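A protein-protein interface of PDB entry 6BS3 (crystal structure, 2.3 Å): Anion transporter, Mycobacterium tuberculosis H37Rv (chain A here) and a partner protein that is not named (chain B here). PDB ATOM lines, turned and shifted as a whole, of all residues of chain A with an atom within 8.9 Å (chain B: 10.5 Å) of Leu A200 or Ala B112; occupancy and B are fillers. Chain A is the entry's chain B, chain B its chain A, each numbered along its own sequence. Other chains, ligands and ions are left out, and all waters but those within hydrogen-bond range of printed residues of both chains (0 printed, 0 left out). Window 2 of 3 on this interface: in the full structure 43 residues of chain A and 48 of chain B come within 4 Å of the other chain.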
ATOM      1  N   LEU A 183      -1.701  21.943 -20.001  1.00  0.00           N
ATOM      2  CA  LEU A 183      -0.888  21.095 -19.093  1.00  0.00           C
ATOM      3  C   LEU A 183      -0.674  21.737 -17.726  1.00  0.00           C
ATOM      4  O   LEU A 183      -0.236  21.025 -16.824  1.00  0.00           O
ATOM      5  CB  LEU A 183       0.444  20.731 -19.750  1.00  0.00           C
ATOM      6  CG  LEU A 183       0.359  20.044 -21.108  1.00  0.00           C
ATOM      7  CD1 LEU A 183       1.730  19.576 -21.541  1.00  0.00           C
ATOM      8  CD2 LEU A 183      -0.608  18.879 -21.068  1.00  0.00           C
ATOM      9  N   ILE A 194      -7.519  14.611 -17.677  1.00  0.00           N
ATOM     10  CA  ILE A 194      -8.741  14.812 -18.456  1.00  0.00           C
ATOM     11  C   ILE A 194      -8.737  13.973 -19.752  1.00  0.00           C
ATOM     12  O   ILE A 194      -9.566  13.064 -19.893  1.00  0.00           O
ATOM     13  CB  ILE A 194      -9.088  16.319 -18.715  1.00  0.00           C
ATOM     14  CG1 ILE A 194      -7.879  17.129 -19.240  1.00  0.00           C
ATOM     15  CG2 ILE A 194      -9.695  16.968 -17.465  1.00  0.00           C
ATOM     16  CD1 ILE A 194      -8.193  18.205 -20.293  1.00  0.00           C
ATOM     17  N   THR A 195      -7.797  14.265 -20.679  1.00  0.00           N
ATOM     18  CA  THR A 195      -7.665  13.585 -21.973  1.00  0.00           C
ATOM     19  C   THR A 195      -6.903  12.254 -21.799  1.00  0.00           C
ATOM     20  O   THR A 195      -6.637  11.830 -20.670  1.00  0.00           O
ATOM     21  CB  THR A 195      -7.024  14.550 -23.020  1.00  0.00           C
ATOM     22  OG1 THR A 195      -7.850  15.706 -23.214  1.00  0.00           O
ATOM     23  CG2 THR A 195      -6.757  13.887 -24.374  1.00  0.00           C
ATOM     24  N   GLY A 196      -6.622  11.588 -22.913  1.00  0.00           N
ATOM     25  CA  GLY A 196      -5.839  10.365 -22.960  1.00  0.00           C
ATOM     26  C   GLY A 196      -4.380  10.750 -23.075  1.00  0.00           C
ATOM     27  O   GLY A 196      -3.564  10.339 -22.250  1.00  0.00           O
ATOM     28  N   VAL A 197      -4.056  11.599 -24.071  1.00  0.00           N
ATOM     29  CA  VAL A 197      -2.699  12.085 -24.341  1.00  0.00           C
ATOM     30  C   VAL A 197      -2.334  13.248 -23.412  1.00  0.00           C
ATOM     31  O   VAL A 197      -1.265  13.205 -22.794  1.00  0.00           O
ATOM     32  CB  VAL A 197      -2.480  12.405 -25.845  1.00  0.00           C
ATOM     33  CG1 VAL A 197      -1.156  13.127 -26.084  1.00  0.00           C
ATOM     34  CG2 VAL A 197      -2.554  11.132 -26.688  1.00  0.00           C
ATOM     35  N   MET A 198      -3.222  14.265 -23.295  1.00  0.00           N
ATOM     36  CA  MET A 198      -3.000  15.427 -22.425  1.00  0.00           C
ATOM     37  C   MET A 198      -2.974  15.016 -20.963  1.00  0.00           C
ATOM     38  O   MET A 198      -2.232  15.616 -20.190  1.00  0.00           O
ATOM     39  CB  MET A 198      -4.038  16.546 -22.633  1.00  0.00           C
ATOM     40  CG  MET A 198      -4.277  16.954 -24.091  1.00  0.00           C
ATOM     41  SD  MET A 198      -2.856  17.523 -25.066  1.00  0.00           S
ATOM     42  CE  MET A 198      -2.317  18.871 -24.120  1.00  0.00           C
ATOM     43  N   GLY A 199      -3.773  14.006 -20.610  1.00  0.00           N
ATOM     44  CA  GLY A 199      -3.852  13.443 -19.266  1.00  0.00           C
ATOM     45  C   GLY A 199      -2.572  12.730 -18.876  1.00  0.00           C
ATOM     46  O   GLY A 199      -2.073  12.924 -17.764  1.00  0.00           O
ATOM     47  N   LEU A 200      -2.018  11.919 -19.809  1.00  0.00           N
ATOM     48  CA  LEU A 200      -0.740  11.208 -19.657  1.00  0.00           C
ATOM     49  C   LEU A 200       0.396  12.225 -19.418  1.00  0.00           C
ATOM     50  O   LEU A 200       1.212  12.023 -18.519  1.00  0.00           O
ATOM     51  CB  LEU A 200      -0.415  10.375 -20.919  1.00  0.00           C
ATOM     52  CG  LEU A 200      -0.888   8.924 -20.979  1.00  0.00           C
ATOM     53  CD1 LEU A 200      -0.725   8.363 -22.388  1.00  0.00           C
ATOM     54  CD2 LEU A 200      -0.148   8.037 -19.974  1.00  0.00           C
ATOM     55  N   ALA A 201       0.424  13.314 -20.219  1.00  0.00           N
ATOM     56  CA  ALA A 201       1.403  14.404 -20.154  1.00  0.00           C
ATOM     57  C   ALA A 201       1.289  15.186 -18.845  1.00  0.00           C
ATOM     58  O   ALA A 201       2.310  15.511 -18.242  1.00  0.00           O
ATOM     59  CB  ALA A 201       1.234  15.337 -21.346  1.00  0.00           C
ATOM     60  N   MET A 202       0.048  15.451 -18.388  1.00  0.00           N
ATOM     61  CA  MET A 202      -0.238  16.150 -17.132  1.00  0.00           C
ATOM     62  C   MET A 202       0.222  15.346 -15.933  1.00  0.00           C
ATOM     63  O   MET A 202       0.764  15.928 -14.989  1.00  0.00           O
ATOM     64  CB  MET A 202      -1.729  16.411 -16.994  1.00  0.00           C
ATOM     65  CG  MET A 202      -2.093  17.847 -17.152  1.00  0.00           C
ATOM     66  SD  MET A 202      -3.869  18.043 -16.908  1.00  0.00           S
ATOM     67  CE  MET A 202      -4.500  17.217 -18.391  1.00  0.00           C
ATOM     68  N   LYS A 203      -0.019  14.013 -15.963  1.00  0.00           N
ATOM     69  CA  LYS A 203       0.377  13.070 -14.921  1.00  0.00           C
ATOM     70  C   LYS A 203       1.908  13.073 -14.822  1.00  0.00           C
ATOM     71  O   LYS A 203       2.434  13.241 -13.721  1.00  0.00           O
ATOM     72  CB  LYS A 203      -0.167  11.655 -15.223  1.00  0.00           C
ATOM     73  CG  LYS A 203       0.068  10.650 -14.102  1.00  0.00           C
ATOM     74  CD  LYS A 203      -0.597   9.311 -14.378  1.00  0.00           C
ATOM     75  CE  LYS A 203      -0.490   8.386 -13.191  1.00  0.00           C
ATOM     76  NZ  LYS A 203      -1.179   7.091 -13.432  1.00  0.00           N
ATOM     77  N   ALA A 204       2.606  12.951 -15.980  1.00  0.00           N
ATOM     78  CA  ALA A 204       4.065  12.956 -16.104  1.00  0.00           C
ATOM     79  C   ALA A 204       4.692  14.211 -15.481  1.00  0.00           C
ATOM     80  O   ALA A 204       5.667  14.088 -14.737  1.00  0.00           O
ATOM     81  CB  ALA A 204       4.467  12.836 -17.569  1.00  0.00           C
ATOM     82  N   LEU A 205       4.114  15.404 -15.758  1.00  0.00           N
ATOM     83  CA  LEU A 205       4.570  16.686 -15.213  1.00  0.00           C
ATOM     84  C   LEU A 205       4.360  16.797 -13.702  1.00  0.00           C
ATOM     85  O   LEU A 205       5.210  17.354 -13.018  1.00  0.00           O
ATOM     86  CB  LEU A 205       3.923  17.877 -15.937  1.00  0.00           C
ATOM     87  CG  LEU A 205       4.293  18.115 -17.408  1.00  0.00           C
ATOM     88  CD1 LEU A 205       4.101  19.571 -17.784  1.00  0.00           C
ATOM     89  CD2 LEU A 205       5.729  17.714 -17.711  1.00  0.00           C
ATOM     90  N   SER A 206       3.235  16.272 -13.190  1.00  0.00           N
ATOM     91  CA  SER A 206       2.883  16.256 -11.763  1.00  0.00           C
ATOM     92  C   SER A 206       3.858  15.364 -10.989  1.00  0.00           C
ATOM     93  O   SER A 206       4.281  15.729  -9.891  1.00  0.00           O
ATOM     94  CB  SER A 206       1.455  15.740 -11.566  1.00  0.00           C
ATOM     95  OG  SER A 206       0.503  16.578 -12.202  1.00  0.00           O
ATOM     96  N   THR A 207       4.211  14.200 -11.581  1.00  0.00           N
ATOM     97  CA  THR A 207       5.124  13.188 -11.049  1.00  0.00           C
ATOM     98  C   THR A 207       6.579  13.695 -10.961  1.00  0.00           C
ATOM     99  O   THR A 207       7.259  13.370  -9.993  1.00  0.00           O
ATOM    100  CB  THR A 207       5.021  11.888 -11.903  1.00  0.00           C
ATOM    101  OG1 THR A 207       3.656  11.479 -12.038  1.00  0.00           O
ATOM    102  CG2 THR A 207       5.801  10.730 -11.319  1.00  0.00           C
ATOM    103  N   GLU B  96      15.456  16.156 -25.068  1.00  0.00           N
ATOM    104  CA  GLU B  96      14.155  15.517 -25.252  1.00  0.00           C
ATOM    105  C   GLU B  96      14.265  14.006 -25.040  1.00  0.00           C
ATOM    106  O   GLU B  96      13.530  13.464 -24.217  1.00  0.00           O
ATOM    107  CB  GLU B  96      13.569  15.902 -26.607  1.00  0.00           C
ATOM    108  CG  GLU B  96      12.328  15.126 -27.001  1.00  0.00           C
ATOM    109  CD  GLU B  96      11.369  15.869 -27.913  1.00  0.00           C
ATOM    110  OE1 GLU B  96      10.288  15.303 -28.187  1.00  0.00           O
ATOM    111  OE2 GLU B  96      11.687  16.999 -28.357  1.00  0.00           O
ATOM    112  N   PHE B  99      15.137  13.272 -21.352  1.00  0.00           N
ATOM    113  CA  PHE B  99      13.940  13.370 -20.507  1.00  0.00           C
ATOM    114  C   PHE B  99      13.096  12.070 -20.556  1.00  0.00           C
ATOM    115  O   PHE B  99      12.648  11.610 -19.505  1.00  0.00           O
ATOM    116  CB  PHE B  99      13.107  14.630 -20.841  1.00  0.00           C
ATOM    117  CG  PHE B  99      11.897  14.851 -19.956  1.00  0.00           C
ATOM    118  CD1 PHE B  99      12.000  14.780 -18.572  1.00  0.00           C
ATOM    119  CD2 PHE B  99      10.652  15.130 -20.508  1.00  0.00           C
ATOM    120  CE1 PHE B  99      10.876  14.960 -17.760  1.00  0.00           C
ATOM    121  CE2 PHE B  99       9.536  15.337 -19.694  1.00  0.00           C
ATOM    122  CZ  PHE B  99       9.655  15.259 -18.325  1.00  0.00           C
ATOM    123  N   LEU B 100      12.943  11.457 -21.760  1.00  0.00           N
ATOM    124  CA  LEU B 100      12.231  10.180 -21.956  1.00  0.00           C
ATOM    125  C   LEU B 100      12.968   9.025 -21.270  1.00  0.00           C
ATOM    126  O   LEU B 100      12.330   8.162 -20.672  1.00  0.00           O
ATOM    127  CB  LEU B 100      12.032   9.850 -23.452  1.00  0.00           C
ATOM    128  CG  LEU B 100      11.297  10.855 -24.341  1.00  0.00           C
ATOM    129  CD1 LEU B 100      11.136  10.304 -25.732  1.00  0.00           C
ATOM    130  CD2 LEU B 100       9.944  11.175 -23.811  1.00  0.00           C
ATOM    131  N   GLU B 101      14.306   9.023 -21.355  1.00  0.00           N
ATOM    132  CA  GLU B 101      15.202   8.054 -20.718  1.00  0.00           C
ATOM    133  C   GLU B 101      14.983   8.091 -19.191  1.00  0.00           C
ATOM    134  O   GLU B 101      14.905   7.055 -18.546  1.00  0.00           O
ATOM    135  CB  GLU B 101      16.648   8.475 -21.023  1.00  0.00           C
ATOM    136  CG  GLU B 101      17.565   7.427 -21.624  1.00  0.00           C
ATOM    137  CD  GLU B 101      18.924   7.956 -22.055  1.00  0.00           C
ATOM    138  OE1 GLU B 101      19.393   8.987 -21.508  1.00  0.00           O
ATOM    139  OE2 GLU B 101      19.524   7.324 -22.955  1.00  0.00           O
ATOM    140  N   TYR B 102      14.873   9.308 -18.631  1.00  0.00           N
ATOM    141  CA  TYR B 102      14.673   9.600 -17.215  1.00  0.00           C
ATOM    142  C   TYR B 102      13.292   9.136 -16.761  1.00  0.00           C
ATOM    143  O   TYR B 102      13.211   8.408 -15.777  1.00  0.00           O
ATOM    144  CB  TYR B 102      14.886  11.106 -17.009  1.00  0.00           C
ATOM    145  CG  TYR B 102      14.578  11.685 -15.650  1.00  0.00           C
ATOM    146  CD1 TYR B 102      15.587  11.879 -14.712  1.00  0.00           C
ATOM    147  CD2 TYR B 102      13.325  12.219 -15.370  1.00  0.00           C
ATOM    148  CE1 TYR B 102      15.334  12.509 -13.492  1.00  0.00           C
ATOM    149  CE2 TYR B 102      13.056  12.843 -14.154  1.00  0.00           C
ATOM    150  CZ  TYR B 102      14.065  12.987 -13.218  1.00  0.00           C
ATOM    151  OH  TYR B 102      13.805  13.610 -12.021  1.00  0.00           O
ATOM    152  N   LEU B 103      12.219   9.522 -17.487  1.00  0.00           N
ATOM    153  CA  LEU B 103      10.843   9.115 -17.184  1.00  0.00           C
ATOM    154  C   LEU B 103      10.708   7.597 -17.149  1.00  0.00           C
ATOM    155  O   LEU B 103      10.091   7.057 -16.231  1.00  0.00           O
ATOM    156  CB  LEU B 103       9.859   9.692 -18.214  1.00  0.00           C
ATOM    157  CG  LEU B 103       9.396  11.126 -18.007  1.00  0.00           C
ATOM    158  CD1 LEU B 103       8.693  11.629 -19.239  1.00  0.00           C
ATOM    159  CD2 LEU B 103       8.456  11.238 -16.835  1.00  0.00           C
ATOM    160  N   ASP B 104      11.317   6.915 -18.128  1.00  0.00           N
ATOM    161  CA  ASP B 104      11.278   5.462 -18.236  1.00  0.00           C
ATOM    162  C   ASP B 104      12.134   4.743 -17.181  1.00  0.00           C
ATOM    163  O   ASP B 104      11.645   3.797 -16.574  1.00  0.00           O
ATOM    164  CB  ASP B 104      11.637   5.010 -19.664  1.00  0.00           C
ATOM    165  CG  ASP B 104      11.496   3.521 -19.919  1.00  0.00           C
ATOM    166  OD1 ASP B 104      10.389   2.970 -19.669  1.00  0.00           O
ATOM    167  OD2 ASP B 104      12.484   2.904 -20.380  1.00  0.00           O
ATOM    168  N   TYR B 107      10.814   6.484 -13.290  1.00  0.00           N
ATOM    169  CA  TYR B 107       9.384   6.521 -12.964  1.00  0.00           C
ATOM    170  C   TYR B 107       8.549   5.510 -13.762  1.00  0.00           C
ATOM    171  O   TYR B 107       7.336   5.418 -13.542  1.00  0.00           O
ATOM    172  CB  TYR B 107       8.834   7.940 -13.201  1.00  0.00           C
ATOM    173  CG  TYR B 107       9.409   9.009 -12.301  1.00  0.00           C
ATOM    174  CD1 TYR B 107       8.846   9.274 -11.056  1.00  0.00           C
ATOM    175  CD2 TYR B 107      10.500   9.774 -12.701  1.00  0.00           C
ATOM    176  CE1 TYR B 107       9.353  10.277 -10.232  1.00  0.00           C
ATOM    177  CE2 TYR B 107      11.029  10.765 -11.878  1.00  0.00           C
ATOM    178  CZ  TYR B 107      10.442  11.023 -10.650  1.00  0.00           C
ATOM    179  OH  TYR B 107      10.950  12.002  -9.833  1.00  0.00           O
ATOM    180  N   ASN B 108       9.194   4.764 -14.692  1.00  0.00           N
ATOM    181  CA  ASN B 108       8.557   3.786 -15.589  1.00  0.00           C
ATOM    182  C   ASN B 108       7.375   4.422 -16.392  1.00  0.00           C
ATOM    183  O   ASN B 108       6.325   3.791 -16.595  1.00  0.00           O
ATOM    184  CB  ASN B 108       8.165   2.486 -14.837  1.00  0.00           C
ATOM    185  CG  ASN B 108       7.949   1.285 -15.735  1.00  0.00           C
ATOM    186  OD1 ASN B 108       8.715   1.014 -16.670  1.00  0.00           O
ATOM    187  ND2 ASN B 108       6.892   0.533 -15.467  1.00  0.00           N
ATOM    188  N   LEU B 109       7.576   5.697 -16.836  1.00  0.00           N
ATOM    189  CA  LEU B 109       6.612   6.501 -17.593  1.00  0.00           C
ATOM    190  C   LEU B 109       7.048   6.652 -19.060  1.00  0.00           C
ATOM    191  O   LEU B 109       6.851   7.707 -19.677  1.00  0.00           O
ATOM    192  CB  LEU B 109       6.406   7.887 -16.929  1.00  0.00           C
ATOM    193  CG  LEU B 109       5.535   7.953 -15.671  1.00  0.00           C
ATOM    194  CD1 LEU B 109       5.820   9.220 -14.883  1.00  0.00           C
ATOM    195  CD2 LEU B 109       4.056   7.894 -16.016  1.00  0.00           C
ATOM    196  N   GLY B 110       7.631   5.580 -19.598  1.00  0.00           N
ATOM    197  CA  GLY B 110       8.080   5.496 -20.983  1.00  0.00           C
ATOM    198  C   GLY B 110       6.938   5.648 -21.967  1.00  0.00           C
ATOM    199  O   GLY B 110       7.122   6.226 -23.041  1.00  0.00           O
ATOM    200  N   ILE B 111       5.741   5.151 -21.583  1.00  0.00           N
ATOM    201  CA  ILE B 111       4.501   5.227 -22.363  1.00  0.00           C
ATOM    202  C   ILE B 111       3.985   6.671 -22.438  1.00  0.00           C
ATOM    203  O   ILE B 111       3.647   7.147 -23.529  1.00  0.00           O
ATOM    204  CB  ILE B 111       3.422   4.210 -21.853  1.00  0.00           C
ATOM    205  CG1 ILE B 111       2.219   4.107 -22.809  1.00  0.00           C
ATOM    206  CG2 ILE B 111       2.973   4.487 -20.408  1.00  0.00           C
ATOM    207  CD1 ILE B 111       2.509   3.296 -24.105  1.00  0.00           C
ATOM    208  N   ALA B 112       3.921   7.350 -21.266  1.00  0.00           N
ATOM    209  CA  ALA B 112       3.501   8.738 -21.105  1.00  0.00           C
ATOM    210  C   ALA B 112       4.478   9.612 -21.889  1.00  0.00           C
ATOM    211  O   ALA B 112       4.031  10.446 -22.668  1.00  0.00           O
ATOM    212  CB  ALA B 112       3.498   9.124 -19.631  1.00  0.00           C
ATOM    213  N   GLY B 113       5.779   9.335 -21.745  1.00  0.00           N
ATOM    214  CA  GLY B 113       6.856  10.021 -22.447  1.00  0.00           C
ATOM    215  C   GLY B 113       6.712  10.005 -23.957  1.00  0.00           C
ATOM    216  O   GLY B 113       6.714  11.065 -24.583  1.00  0.00           O
ATOM    217  N   ARG B 114       6.560   8.803 -24.552  1.00  0.00           N
ATOM    218  CA  ARG B 114       6.362   8.601 -25.996  1.00  0.00           C
ATOM    219  C   ARG B 114       5.129   9.331 -26.540  1.00  0.00           C
ATOM    220  O   ARG B 114       5.152   9.775 -27.693  1.00  0.00           O
ATOM    221  CB  ARG B 114       6.305   7.106 -26.351  1.00  0.00           C
ATOM    222  CG  ARG B 114       7.665   6.532 -26.696  1.00  0.00           C
ATOM    223  CD  ARG B 114       7.590   5.039 -26.924  1.00  0.00           C
ATOM    224  NE  ARG B 114       8.162   4.298 -25.799  1.00  0.00           N
ATOM    225  CZ  ARG B 114       7.451   3.627 -24.898  1.00  0.00           C
ATOM    226  NH1 ARG B 114       6.126   3.579 -24.990  1.00  0.00           N
ATOM    227  NH2 ARG B 114       8.058   2.995 -23.903  1.00  0.00           N
ATOM    228  N   ALA B 115       4.068   9.461 -25.713  1.00  0.00           N
ATOM    229  CA  ALA B 115       2.837  10.169 -26.065  1.00  0.00           C
ATOM    230  C   ALA B 115       3.078  11.691 -26.066  1.00  0.00           C
ATOM    231  O   ALA B 115       2.524  12.396 -26.911  1.00  0.00           O
ATOM    232  CB  ALA B 115       1.728   9.813 -25.086  1.00  0.00           C
ATOM    233  N   MET B 116       3.918  12.182 -25.129  1.00  0.00           N
ATOM    234  CA  MET B 116       4.304  13.590 -24.969  1.00  0.00           C
ATOM    235  C   MET B 116       5.128  14.096 -26.156  1.00  0.00           C
ATOM    236  O   MET B 116       4.996  15.257 -26.535  1.00  0.00           O
ATOM    237  CB  MET B 116       5.137  13.780 -23.696  1.00  0.00           C
ATOM    238  CG  MET B 116       4.371  13.599 -22.425  1.00  0.00           C
ATOM    239  SD  MET B 116       5.503  13.756 -21.040  1.00  0.00           S
ATOM    240  CE  MET B 116       5.482  15.538 -20.805  1.00  0.00           C
ATOM    241  N   ARG B 117       6.008  13.240 -26.702  1.00  0.00           N
ATOM    242  CA  ARG B 117       6.866  13.549 -27.848  1.00  0.00           C
ATOM    243  C   ARG B 117       5.993  13.858 -29.093  1.00  0.00           C
ATOM    244  O   ARG B 117       6.247  14.836 -29.792  1.00  0.00           O
ATOM    245  CB  ARG B 117       7.851  12.386 -28.092  1.00  0.00           C
ATOM    246  CG  ARG B 117       8.749  12.540 -29.322  1.00  0.00           C
ATOM    247  CD  ARG B 117       9.639  11.333 -29.572  1.00  0.00           C
ATOM    248  NE  ARG B 117       8.877  10.114 -29.851  1.00  0.00           N
ATOM    249  CZ  ARG B 117       9.314   8.887 -29.580  1.00  0.00           C
ATOM    250  NH1 ARG B 117      10.515   8.705 -29.043  1.00  0.00           N
ATOM    251  NH2 ARG B 117       8.553   7.833 -29.841  1.00  0.00           N
ATOM    252  N   ARG B 118       4.917  13.076 -29.292  1.00  0.00           N
ATOM    253  CA  ARG B 118       3.969  13.209 -30.403  1.00  0.00           C
ATOM    254  C   ARG B 118       3.111  14.489 -30.360  1.00  0.00           C
ATOM    255  O   ARG B 118       2.418  14.756 -31.343  1.00  0.00           O
ATOM    256  CB  ARG B 118       3.069  11.955 -30.518  1.00  0.00           C
ATOM    257  CG  ARG B 118       3.832  10.651 -30.730  1.00  0.00           C
ATOM    258  CD  ARG B 118       2.887   9.469 -30.840  1.00  0.00           C
ATOM    259  NE  ARG B 118       3.565   8.201 -30.554  1.00  0.00           N
ATOM    260  CZ  ARG B 118       3.240   7.373 -29.561  1.00  0.00           C
ATOM    261  NH1 ARG B 118       2.223   7.658 -28.755  1.00  0.00           N
ATOM    262  NH2 ARG B 118       3.920   6.250 -29.377  1.00  0.00           N
ATOM    263  N   ILE B 119       3.140  15.263 -29.237  1.00  0.00           N
ATOM    264  CA  ILE B 119       2.370  16.512 -29.047  1.00  0.00           C
ATOM    265  C   ILE B 119       3.270  17.698 -28.592  1.00  0.00           C
ATOM    266  O   ILE B 119       2.749  18.724 -28.136  1.00  0.00           O
ATOM    267  CB  ILE B 119       1.113  16.336 -28.125  1.00  0.00           C
ATOM    268  CG1 ILE B 119       1.481  15.883 -26.694  1.00  0.00           C
ATOM    269  CG2 ILE B 119       0.062  15.415 -28.755  1.00  0.00           C
ATOM    270  CD1 ILE B 119       0.725  16.603 -25.582  1.00  0.00           C
ATOM    271  N   GLY B 120       4.594  17.527 -28.724  1.00  0.00           N
ATOM    272  CA  GLY B 120       5.620  18.510 -28.382  1.00  0.00           C
ATOM    273  C   GLY B 120       5.714  18.896 -26.919  1.00  0.00           C
ATOM    274  O   GLY B 120       6.230  19.974 -26.605  1.00  0.00           O
ATOM    275  N   ALA B 121       5.255  18.007 -26.007  1.00  0.00           N
ATOM    276  CA  ALA B 121       5.203  18.250 -24.555  1.00  0.00           C
ATOM    277  C   ALA B 121       6.530  18.067 -23.822  1.00  0.00           C
ATOM    278  O   ALA B 121       6.666  18.531 -22.685  1.00  0.00           O
ATOM    279  CB  ALA B 121       4.114  17.396 -23.913  1.00  0.00           C
ATOM    280  N   VAL B 122       7.502  17.393 -24.453  1.00  0.00           N
ATOM    281  CA  VAL B 122       8.830  17.163 -23.861  1.00  0.00           C
ATOM    282  C   VAL B 122       9.642  18.451 -24.027  1.00  0.00           C
ATOM    283  O   VAL B 122      10.296  18.882 -23.074  1.00  0.00           O
ATOM    284  CB  VAL B 122       9.542  15.906 -24.438  1.00  0.00           C
ATOM    285  CG1 VAL B 122      10.862  15.636 -23.728  1.00  0.00           C
ATOM    286  CG2 VAL B 122       8.637  14.678 -24.368  1.00  0.00           C
ATOM    287  N   ALA B 125       8.090  20.958 -21.370  1.00  0.00           N
ATOM    288  CA  ALA B 125       8.543  20.610 -20.008  1.00  0.00           C
ATOM    289  C   ALA B 125       9.999  20.994 -19.741  1.00  0.00           C
ATOM    290  O   ALA B 125      10.296  21.547 -18.676  1.00  0.00           O
ATOM    291  CB  ALA B 125       8.342  19.120 -19.754  1.00  0.00           C
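Among the printed residues, merely in contact across the chains: Thr A207 with Tyr B107, Leu A205 with Ala B125, Val A197 with Ile B119, Met A198 with Ile B119, Ala A204 with Met B116, Ala A201 with Met B116, Leu A205 with Met B116, Leu A200 with Ala B112, Val A197 with Ala B115, Thr A207 with Leu B109 and Leu A200 with Ala B115.
Hydrophobic or aromatic side chains of chain A within 4 Å of the printed part of chain B: Val A197, Met A198, Leu A200, Ala A201, Ala A204 and Leu A205. Of the 24 printed residues of chain B, 7 touch a printed residue of chain A. Hydrophobic or aromatic side chains of chain B within 4 Å of the printed part of chain A: Tyr B107, Leu B109, Ala B112, Ala B115, Met B116, Ile B119 and Ala B125. Among the printed residues, 11 pairs touch across the chains. Among the printed residues, no Asp or Glu carboxylate lies within 4 Å of a Lys or Arg side-chain nitrogen of the other chain.
The backbone carbonyl oxygen (O) of Leu B103 is in hydrogen-bond range of the backbone NH (N) of Leu B109 (2.9 Å). The backbone NH (N) of Ala B121 sits at hydrogen-bond distance from the backbone carbonyl oxygen (O) of Met B116, 2.8 Å away. The backbone carbonyl oxygen (O) of Lys A203 is in hydrogen-bond range of the side-chain hydroxyl (OG1) of Thr A207, 2.7 Å away.
Ile A194 touches none of the printed residues of chain B. Gly A199 touches none of the printed residues of chain B. Leu A200 touches just these residues of chain B: Ala B112 (3.8 Å) and Ala B115 (3.9 Å). Printed residues of chain B within 4 Å of Ala A201: Met B116. Ala A204 touches one residue of chain B. Of the printed residues of chain A, Tyr B107 touches Thr A207. Ile B111 touches none of the printed residues of chain A. Ala B112 touches just one residue of chain A: Leu A200 (3.8 Å). No residue of chain A comes within 4 Å of Gly B113. Of the printed residues of chain A, Ala B115 touches Val A197 and Leu A200. The nearest residue of chain B that does not touch Leu A200 is Ile B111 (4.7 Å). The nearest residue of chain A that does not touch Ala B112 is Ala A204 (4.4 Å). The nearest printed residue of chain A that does not touch Ala B125 is Leu A183 (6.5 Å).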
